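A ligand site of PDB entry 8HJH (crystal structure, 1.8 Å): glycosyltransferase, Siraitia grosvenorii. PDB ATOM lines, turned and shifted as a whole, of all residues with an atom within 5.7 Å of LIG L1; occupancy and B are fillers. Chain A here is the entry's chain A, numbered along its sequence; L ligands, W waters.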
ATOM      1  N   PRO A 125      34.784  14.598  28.892  1.00  0.00           N
ATOM      2  CA  PRO A 125      34.817  13.685  27.747  1.00  0.00           C
ATOM      3  C   PRO A 125      36.195  13.104  27.473  1.00  0.00           C
ATOM      4  O   PRO A 125      36.288  12.004  26.897  1.00  0.00           O
ATOM      5  CB  PRO A 125      34.438  14.579  26.558  1.00  0.00           C
ATOM      6  CG  PRO A 125      33.717  15.718  27.180  1.00  0.00           C
ATOM      7  CD  PRO A 125      34.356  15.954  28.512  1.00  0.00           C
ATOM      8  N   TRP A 126      37.267  13.850  27.802  1.00  0.00           N
ATOM      9  CA  TRP A 126      38.614  13.349  27.593  1.00  0.00           C
ATOM     10  C   TRP A 126      38.894  12.076  28.392  1.00  0.00           C
ATOM     11  O   TRP A 126      39.789  11.296  28.000  1.00  0.00           O
ATOM     12  CB  TRP A 126      39.653  14.423  27.927  1.00  0.00           C
ATOM     13  CG  TRP A 126      39.421  15.105  29.206  1.00  0.00           C
ATOM     14  CD1 TRP A 126      38.678  16.227  29.404  1.00  0.00           C
ATOM     15  CD2 TRP A 126      39.957  14.746  30.457  1.00  0.00           C
ATOM     16  NE1 TRP A 126      38.692  16.570  30.720  1.00  0.00           N
ATOM     17  CE2 TRP A 126      39.468  15.674  31.398  1.00  0.00           C
ATOM     18  CE3 TRP A 126      40.773  13.714  30.885  1.00  0.00           C
ATOM     19  CZ2 TRP A 126      39.831  15.648  32.733  1.00  0.00           C
ATOM     20  CZ3 TRP A 126      41.119  13.659  32.203  1.00  0.00           C
ATOM     21  CH2 TRP A 126      40.633  14.619  33.133  1.00  0.00           C
ATOM     22  N   ARG A 129      38.206   8.736  26.723  1.00  0.00           N
ATOM     23  CA  ARG A 129      39.111   8.664  25.577  1.00  0.00           C
ATOM     24  C   ARG A 129      40.524   8.258  25.997  1.00  0.00           C
ATOM     25  O   ARG A 129      41.142   7.428  25.323  1.00  0.00           O
ATOM     26  CB  ARG A 129      39.159  10.020  24.861  1.00  0.00           C
ATOM     27  CG  ARG A 129      37.814  10.333  24.135  1.00  0.00           C
ATOM     28  CD  ARG A 129      37.729   9.615  22.806  1.00  0.00           C
ATOM     29  NE  ARG A 129      38.783  10.139  21.930  1.00  0.00           N
ATOM     30  CZ  ARG A 129      39.354   9.477  20.913  1.00  0.00           C
ATOM     31  NH1 ARG A 129      40.297  10.065  20.194  1.00  0.00           N
ATOM     32  NH2 ARG A 129      38.971   8.242  20.599  1.00  0.00           N
ATOM     33  N   LEU A 153      16.815  15.654  27.562  1.00  0.00           N
ATOM     34  CA  LEU A 153      16.987  14.856  26.349  1.00  0.00           C
ATOM     35  C   LEU A 153      15.678  14.666  25.582  1.00  0.00           C
ATOM     36  O   LEU A 153      15.708  14.505  24.358  1.00  0.00           O
ATOM     37  CB  LEU A 153      17.569  13.488  26.709  1.00  0.00           C
ATOM     38  CG  LEU A 153      18.073  12.592  25.575  1.00  0.00           C
ATOM     39  CD1 LEU A 153      18.996  13.326  24.598  1.00  0.00           C
ATOM     40  CD2 LEU A 153      18.791  11.437  26.262  1.00  0.00           C
ATOM     41  N   ILE A 156      14.947  16.734  22.323  1.00  0.00           N
ATOM     42  CA  ILE A 156      15.787  16.413  21.158  1.00  0.00           C
ATOM     43  C   ILE A 156      15.078  15.382  20.280  1.00  0.00           C
ATOM     44  O   ILE A 156      15.042  15.508  19.052  1.00  0.00           O
ATOM     45  CB  ILE A 156      17.184  15.932  21.625  1.00  0.00           C
ATOM     46  CG1 ILE A 156      17.800  16.908  22.653  1.00  0.00           C
ATOM     47  CG2 ILE A 156      18.122  15.618  20.435  1.00  0.00           C
ATOM     48  CD1 ILE A 156      17.746  18.384  22.216  1.00  0.00           C
ATOM     49  N   HIS A 157      14.494  14.359  20.898  1.00  0.00           N
ATOM     50  CA  HIS A 157      13.810  13.337  20.131  1.00  0.00           C
ATOM     51  C   HIS A 157      12.352  13.669  19.850  1.00  0.00           C
ATOM     52  O   HIS A 157      11.815  13.237  18.822  1.00  0.00           O
ATOM     53  CB  HIS A 157      13.896  11.997  20.852  1.00  0.00           C
ATOM     54  CG  HIS A 157      15.307  11.544  21.104  1.00  0.00           C
ATOM     55  ND1 HIS A 157      16.003  10.763  20.208  1.00  0.00           N
ATOM     56  CD2 HIS A 157      16.151  11.783  22.138  1.00  0.00           C
ATOM     57  CE1 HIS A 157      17.218  10.522  20.689  1.00  0.00           C
ATOM     58  NE2 HIS A 157      17.332  11.140  21.854  1.00  0.00           N
ATOM     59  N   LYS A 191      27.144  22.645  22.345  1.00  0.00           N
ATOM     60  CA  LYS A 191      28.422  21.912  22.518  1.00  0.00           C
ATOM     61  C   LYS A 191      28.540  21.404  23.958  1.00  0.00           C
ATOM     62  O   LYS A 191      28.982  20.257  24.134  1.00  0.00           O
ATOM     63  CB  LYS A 191      29.607  22.809  22.150  1.00  0.00           C
ATOM     64  CG  LYS A 191      29.771  23.092  20.660  1.00  0.00           C
ATOM     65  CD  LYS A 191      30.955  23.975  20.335  1.00  0.00           C
ATOM     66  CE  LYS A 191      32.262  23.382  20.804  1.00  0.00           C
ATOM     67  NZ  LYS A 191      33.417  24.237  20.436  1.00  0.00           N
ATOM     68  N   GLY A 193      26.108  20.633  25.994  1.00  0.00           N
ATOM     69  CA  GLY A 193      25.176  19.495  26.103  1.00  0.00           C
ATOM     70  C   GLY A 193      25.728  18.254  25.421  1.00  0.00           C
ATOM     71  O   GLY A 193      25.565  17.157  25.977  1.00  0.00           O
ATOM     72  N   GLU A 194      26.347  18.417  24.250  1.00  0.00           N
ATOM     73  CA  GLU A 194      26.923  17.265  23.497  1.00  0.00           C
ATOM     74  C   GLU A 194      28.044  16.629  24.306  1.00  0.00           C
ATOM     75  O   GLU A 194      28.126  15.391  24.325  1.00  0.00           O
ATOM     76  CB  GLU A 194      27.439  17.731  22.129  1.00  0.00           C
ATOM     77  CG  GLU A 194      26.332  18.034  21.135  1.00  0.00           C
ATOM     78  CD  GLU A 194      26.809  18.670  19.843  1.00  0.00           C
ATOM     79  OE1 GLU A 194      26.016  18.726  18.892  1.00  0.00           O
ATOM     80  OE2 GLU A 194      27.976  19.114  19.795  1.00  0.00           O
ATOM     81  N   ALA A 195      28.871  17.448  24.957  1.00  0.00           N
ATOM     82  CA  ALA A 195      29.992  16.921  25.774  1.00  0.00           C
ATOM     83  C   ALA A 195      29.427  16.139  26.965  1.00  0.00           C
ATOM     84  O   ALA A 195      29.961  15.056  27.257  1.00  0.00           O
ATOM     85  CB  ALA A 195      30.866  18.061  26.236  1.00  0.00           C
ATOM     86  N   LEU A 197      26.408  14.661  27.156  1.00  0.00           N
ATOM     87  CA  LEU A 197      25.779  13.444  26.682  1.00  0.00           C
ATOM     88  C   LEU A 197      26.828  12.440  26.225  1.00  0.00           C
ATOM     89  O   LEU A 197      26.639  11.239  26.387  1.00  0.00           O
ATOM     90  CB  LEU A 197      24.776  13.773  25.596  1.00  0.00           C
ATOM     91  CG  LEU A 197      23.496  14.438  26.096  1.00  0.00           C
ATOM     92  CD1 LEU A 197      22.639  14.752  24.850  1.00  0.00           C
ATOM     93  CD2 LEU A 197      22.676  13.567  27.047  1.00  0.00           C
ATOM     94  N   TYR A 198      27.939  12.912  25.651  1.00  0.00           N
ATOM     95  CA  TYR A 198      28.985  11.984  25.211  1.00  0.00           C
ATOM     96  C   TYR A 198      29.523  11.185  26.398  1.00  0.00           C
ATOM     97  O   TYR A 198      29.793   9.972  26.285  1.00  0.00           O
ATOM     98  CB  TYR A 198      30.133  12.742  24.529  1.00  0.00           C
ATOM     99  CG  TYR A 198      31.278  11.806  24.163  1.00  0.00           C
ATOM    100  CD1 TYR A 198      31.170  10.935  23.100  1.00  0.00           C
ATOM    101  CD2 TYR A 198      32.455  11.773  24.954  1.00  0.00           C
ATOM    102  CE1 TYR A 198      32.197  10.057  22.783  1.00  0.00           C
ATOM    103  CE2 TYR A 198      33.502  10.902  24.618  1.00  0.00           C
ATOM    104  CZ  TYR A 198      33.357  10.062  23.541  1.00  0.00           C
ATOM    105  OH  TYR A 198      34.353   9.184  23.195  1.00  0.00           O
ATOM    106  N   HIS A 201      27.020   8.496  26.892  1.00  0.00           N
ATOM    107  CA  HIS A 201      26.974   7.623  25.721  1.00  0.00           C
ATOM    108  C   HIS A 201      28.246   6.801  25.569  1.00  0.00           C
ATOM    109  O   HIS A 201      28.171   5.632  25.146  1.00  0.00           O
ATOM    110  CB  HIS A 201      26.723   8.494  24.503  1.00  0.00           C
ATOM    111  CG  HIS A 201      26.740   7.760  23.212  1.00  0.00           C
ATOM    112  ND1 HIS A 201      25.761   6.869  22.850  1.00  0.00           N
ATOM    113  CD2 HIS A 201      27.557   7.872  22.132  1.00  0.00           C
ATOM    114  CE1 HIS A 201      25.989   6.425  21.623  1.00  0.00           C
ATOM    115  NE2 HIS A 201      27.076   7.019  21.170  1.00  0.00           N
ATOM    116  N   VAL A 225      15.946   4.096  27.384  1.00  0.00           N
ATOM    117  CA  VAL A 225      15.451   3.944  26.011  1.00  0.00           C
ATOM    118  C   VAL A 225      16.059   4.996  25.095  1.00  0.00           C
ATOM    119  O   VAL A 225      16.551   4.682  23.996  1.00  0.00           O
ATOM    120  CB  VAL A 225      13.916   4.047  25.993  1.00  0.00           C
ATOM    121  CG1 VAL A 225      13.410   4.208  24.559  1.00  0.00           C
ATOM    122  CG2 VAL A 225      13.289   2.843  26.696  1.00  0.00           C
ATOM    123  N   LEU A 226      16.038   6.261  25.537  1.00  0.00           N
ATOM    124  CA  LEU A 226      16.552   7.373  24.693  1.00  0.00           C
ATOM    125  C   LEU A 226      18.028   7.169  24.354  1.00  0.00           C
ATOM    126  O   LEU A 226      18.401   7.410  23.194  1.00  0.00           O
ATOM    127  CB  LEU A 226      16.323   8.693  25.426  1.00  0.00           C
ATOM    128  CG  LEU A 226      14.868   9.122  25.604  1.00  0.00           C
ATOM    129  CD1 LEU A 226      14.773  10.403  26.416  1.00  0.00           C
ATOM    130  CD2 LEU A 226      14.171   9.285  24.261  1.00  0.00           C
ATOM    131  N   LEU A 227      18.838   6.792  25.340  1.00  0.00           N
ATOM    132  CA  LEU A 227      20.307   6.641  25.119  1.00  0.00           C
ATOM    133  C   LEU A 227      20.635   5.252  24.567  1.00  0.00           C
ATOM    134  O   LEU A 227      21.793   5.055  24.146  1.00  0.00           O
ATOM    135  CB  LEU A 227      21.039   6.866  26.440  1.00  0.00           C
ATOM    136  CG  LEU A 227      21.122   8.312  26.911  1.00  0.00           C
ATOM    137  CD1 LEU A 227      21.764   8.389  28.286  1.00  0.00           C
ATOM    138  CD2 LEU A 227      21.897   9.153  25.913  1.00  0.00           C
ATOM    139  N   ASN A 228      19.672   4.327  24.583  1.00  0.00           N
ATOM    140  CA  ASN A 228      19.944   2.916  24.156  1.00  0.00           C
ATOM    141  C   ASN A 228      21.094   2.380  25.014  1.00  0.00           C
ATOM    142  O   ASN A 228      21.950   1.651  24.478  1.00  0.00           O
ATOM    143  CB  ASN A 228      20.188   2.794  22.656  1.00  0.00           C
ATOM    144  CG  ASN A 228      19.950   1.402  22.118  1.00  0.00           C
ATOM    145  OD1 ASN A 228      20.386   1.063  21.021  1.00  0.00           O
ATOM    146  ND2 ASN A 228      19.269   0.576  22.895  1.00  0.00           N
HETATM  147  O1  LIG L   1      31.522  16.274  22.227  1.00  0.00           O
HETATM  148  O2  LIG L   1      16.555   6.706  16.412  1.00  0.00           O
HETATM  149  O3  LIG L   1      40.842  15.604  23.682  1.00  0.00           O
HETATM  150  O4  LIG L   1      41.487  12.228  21.787  1.00  0.00           O
HETATM  151  C1  LIG L   1      25.050  11.761  21.465  1.00  0.00           C
HETATM  152  C2  LIG L   1      25.537  12.908  20.547  1.00  0.00           C
HETATM  153  C3  LIG L   1      23.525  11.693  21.619  1.00  0.00           C
HETATM  154  C4  LIG L   1      22.655  11.880  20.293  1.00  0.00           C
HETATM  155  C5  LIG L   1      27.073  12.676  20.410  1.00  0.00           C
HETATM  156  C6  LIG L   1      24.461  13.606  19.665  1.00  0.00           C
HETATM  157  C7  LIG L   1      26.133  11.688  22.586  1.00  0.00           C
HETATM  158  C8  LIG L   1      23.333  12.760  19.211  1.00  0.00           C
HETATM  159  C9  LIG L   1      22.210  10.560  19.570  1.00  0.00           C
HETATM  160  C10 LIG L   1      27.491  12.277  21.870  1.00  0.00           C
HETATM  161  C11 LIG L   1      23.095  10.495  22.562  1.00  0.00           C
HETATM  162  C12 LIG L   1      25.501  10.497  20.674  1.00  0.00           C
HETATM  163  C13 LIG L   1      25.455  13.985  21.659  1.00  0.00           C
HETATM  164  C14 LIG L   1      28.061  13.647  19.897  1.00  0.00           C
HETATM  165  C15 LIG L   1      22.436   9.212  20.367  1.00  0.00           C
HETATM  166  C16 LIG L   1      21.381  12.604  20.750  1.00  0.00           C
HETATM  167  C17 LIG L   1      20.836  10.636  18.931  1.00  0.00           C
HETATM  168  C18 LIG L   1      22.469   9.208  21.883  1.00  0.00           C
HETATM  169  C19 LIG L   1      21.924   7.968  19.592  1.00  0.00           C
HETATM  170  C20 LIG L   1      20.656   9.482  18.060  1.00  0.00           C
HETATM  171  C21 LIG L   1      20.599   8.171  18.850  1.00  0.00           C
HETATM  172  C22 LIG L   1      28.996  14.050  21.011  1.00  0.00           C
HETATM  173  C23 LIG L   1      27.556  14.892  19.114  1.00  0.00           C
HETATM  174  C24 LIG L   1      21.791   6.806  20.596  1.00  0.00           C
HETATM  175  C25 LIG L   1      23.046   7.594  18.578  1.00  0.00           C
HETATM  176  C26 LIG L   1      30.256  14.851  20.456  1.00  0.00           C
HETATM  177  C27 LIG L   1      31.593  14.242  20.931  1.00  0.00           C
HETATM  178  C28 LIG L   1      18.278   7.672  19.587  1.00  0.00           C
HETATM  179  C29 LIG L   1      32.390  15.383  21.575  1.00  0.00           C
HETATM  180  C30 LIG L   1      17.835   7.682  18.123  1.00  0.00           C
HETATM  181  C31 LIG L   1      16.578   6.988  17.852  1.00  0.00           C
HETATM  182  C32 LIG L   1      33.162  16.185  20.497  1.00  0.00           C
HETATM  183  C33 LIG L   1      33.351  14.866  22.657  1.00  0.00           C
HETATM  184  C34 LIG L   1      16.799   5.790  20.060  1.00  0.00           C
HETATM  185  C35 LIG L   1      16.408   5.718  18.577  1.00  0.00           C
HETATM  186  C36 LIG L   1      33.085  12.522  20.124  1.00  0.00           C
HETATM  187  C37 LIG L   1      32.910  11.405  19.109  1.00  0.00           C
HETATM  188  C38 LIG L   1      15.778   6.611  20.792  1.00  0.00           C
HETATM  189  C39 LIG L   1      34.025  10.453  19.189  1.00  0.00           C
HETATM  190  C40 LIG L   1      35.537  12.486  19.465  1.00  0.00           C
HETATM  191  C41 LIG L   1      35.345  11.067  18.925  1.00  0.00           C
HETATM  192  C42 LIG L   1      36.845  12.560  20.235  1.00  0.00           C
HETATM  193  C43 LIG L   1      30.970  10.181  18.504  1.00  0.00           C
HETATM  194  C44 LIG L   1      30.154   9.041  19.091  1.00  0.00           C
HETATM  195  C45 LIG L   1      29.306   8.492  18.036  1.00  0.00           C
HETATM  196  C46 LIG L   1      28.744  10.926  17.574  1.00  0.00           C
HETATM  197  C47 LIG L   1      28.266   9.453  17.654  1.00  0.00           C
HETATM  198  C48 LIG L   1      37.677  14.142  21.824  1.00  0.00           C
HETATM  199  C49 LIG L   1      37.370  14.724  23.198  1.00  0.00           C
HETATM  200  C50 LIG L   1      28.400  11.490  16.212  1.00  0.00           C
HETATM  201  C51 LIG L   1      38.485  15.511  23.732  1.00  0.00           C
HETATM  202  C52 LIG L   1      39.844  13.518  22.936  1.00  0.00           C
HETATM  203  C53 LIG L   1      39.716  14.729  23.880  1.00  0.00           C
HETATM  204  C54 LIG L   1      41.274  13.453  22.450  1.00  0.00           C
HETATM  205  O5  LIG L   1      22.416  13.513  18.634  1.00  0.00           O
HETATM  206  O6  LIG L   1      19.542   8.249  19.825  1.00  0.00           O
HETATM  207  O7  LIG L   1      32.274  13.627  19.832  1.00  0.00           O
HETATM  208  O8  LIG L   1      18.144   6.368  20.248  1.00  0.00           O
HETATM  209  O9  LIG L   1      17.525   9.041  17.810  1.00  0.00           O
HETATM  210  O10 LIG L   1      34.468  12.996  20.320  1.00  0.00           O
HETATM  211  O11 LIG L   1      15.011   5.379  18.475  1.00  0.00           O
HETATM  212  O12 LIG L   1      31.695  10.740  19.541  1.00  0.00           O
HETATM  213  O13 LIG L   1      15.032   5.769  21.643  1.00  0.00           O
HETATM  214  O14 LIG L   1      33.894   9.412  18.158  1.00  0.00           O
HETATM  215  O15 LIG L   1      36.363  10.200  19.468  1.00  0.00           O
HETATM  216  O16 LIG L   1      36.665  13.241  21.488  1.00  0.00           O
HETATM  217  O17 LIG L   1      30.166  11.219  17.861  1.00  0.00           O
HETATM  218  O18 LIG L   1      31.059   8.026  19.566  1.00  0.00           O
HETATM  219  O19 LIG L   1      28.640   7.281  18.546  1.00  0.00           O
HETATM  220  O20 LIG L   1      38.981  13.482  21.746  1.00  0.00           O
HETATM  221  O21 LIG L   1      27.699   9.037  16.397  1.00  0.00           O
HETATM  222  O22 LIG L   1      36.292  15.659  23.032  1.00  0.00           O
HETATM  223  O23 LIG L   1      29.332  12.475  15.826  1.00  0.00           O
HETATM  224  O24 LIG L   1      38.043  15.996  25.052  1.00  0.00           O
HETATM  225  O1  LG2 L   2      14.338   7.234  13.431  1.00  0.00           O
HETATM  226  C1  LG2 L   2      13.302   8.185  13.402  1.00  0.00           C
HETATM  227  C2  LG2 L   2      12.453   7.995  12.140  1.00  0.00           C
HETATM  228  C3  LG2 L   2      13.879   9.622  13.483  1.00  0.00           C
HETATM  229  O2  LG2 L   2      15.028   9.764  12.690  1.00  0.00           O
HETATM  230  C4  LG2 L   2      15.884  10.869  12.937  1.00  0.00           C
HETATM  231  O3  LG2 L   2      24.575  10.855  15.891  1.00  0.00           O
HETATM  232  C5  LG2 L   2      23.931  11.776  14.974  1.00  0.00           C
HETATM  233  C6  LG2 L   2      23.375  13.146  15.423  1.00  0.00           C
HETATM  234  O4  LG2 L   2      22.244  13.508  14.632  1.00  0.00           O
HETATM  235  C7  LG2 L   2      21.140  12.642  14.709  1.00  0.00           C
HETATM  236  C8  LG2 L   2      19.887  13.356  14.178  1.00  0.00           C
HETATM  237  O5  LG2 L   2      18.737  13.298  15.033  1.00  0.00           O
HETATM  238  C9  LG2 L   2      18.661  12.342  16.045  1.00  0.00           C
HETATM  239  C10 LG2 L   2      17.190  11.935  16.251  1.00  0.00           C
HETATM  240  O6  LG2 L   2      16.744  11.088  15.195  1.00  0.00           O
HETATM  241  C11 LG2 L   2      15.712  11.516  14.329  1.00  0.00           C
HETATM  242  C12 LG2 L   2      15.669  11.923  11.847  1.00  0.00           C
HETATM  243  C13 LG2 L   2      16.284  13.161  16.379  1.00  0.00           C
HETATM  244  C14 LG2 L   2      19.540  12.841  12.788  1.00  0.00           C
HETATM  245  C15 LG2 L   2      24.461  14.252  15.371  1.00  0.00           C
HETATM  246  O   HOH W   1      38.522  10.641  17.839  1.00  0.00           O
HETATM  247  O   HOH W   2      36.875  17.437  21.070  1.00  0.00           O
HETATM  248  O   HOH W   3      35.463   7.489  20.052  1.00  0.00           O
HETATM  249  O   HOH W   4      26.304   5.999  17.671  1.00  0.00           O
HETATM  250  O   HOH W   5      31.136  14.142  17.303  1.00  0.00           O
HETATM  251  O   HOH W   6      41.704  12.413  25.758  1.00  0.00           O
HETATM  252  O   HOH W   7      42.551  14.827  25.800  1.00  0.00           O
HETATM  253  O   HOH W   8      39.567  18.194  25.967  1.00  0.00           O
HETATM  254  O   HOH W   9      33.900  10.526  15.581  1.00  0.00           O
HETATM  255  O   HOH W  10      30.860  19.266  22.550  1.00  0.00           O
HETATM  256  O   HOH W  11      28.531   7.153  14.528  1.00  0.00           O
HETATM  257  O   HOH W  12      19.730   3.893  19.544  1.00  0.00           O
HETATM  258  O   HOH W  13      19.546   9.888  22.755  1.00  0.00           O
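NH1 of Arg 129 lies within hydrogen-bond range of O4 of LIG L1 (2.9 Å).
O of Val 225 sits at hydrogen-bond distance from O13 of LIG L1, at 3.0 Å.
An oxygen (O19) of LIG L1 is in hydrogen-bond range of a ring nitrogen (NE2) of His 201.
O9 of LIG L1 sits close to ND1 of His 157 (3.3 Å).
O9 of LIG L1 sits close to O6 of LG2 L2 (3.4 Å).
O8 of LIG L1 lies close to O of Leu 226 (3.1 Å).
Trp 126 touches LIG L1 (N to O24, 3.6 Å).
Glu 194 touches LIG L1 (O to C22, 3.7 Å).
CA of Ala 195 touches O1 of LIG L1, at 3.9 Å.
Leu 197 touches LIG L1 (C to C7, 3.8 Å).
Tyr 198 touches LIG L1 (CE1 to O12, 3.4 Å).
CD2 of Leu 227 touches C11 of LIG L1 (3.8 Å).
Hydrophobic or aromatic side chains within 4 Å of LIG L1: Trp 126, His 157, Leu 197, Tyr 198, His 201, Val 225 and Leu 227.
Of the 17 residues printed, 11 come within 4 Å of LIG L1.
Water W1 bridges O15 of LIG L1 and NH1 of Arg 129.
Water W12 bridges an oxygen (O8) of LIG L1 (3.0 Å) and the side-chain amide oxygen (OD1) of Asn 228 (3.3 Å).
Water W10 bridges the backbone carbonyl oxygen of Lys 191 and an oxygen (O1) of LIG L1.
Water W13 lies within hydrogen-bond range of NE2 of His 157, O of Leu 226 and O6 of LIG L1.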
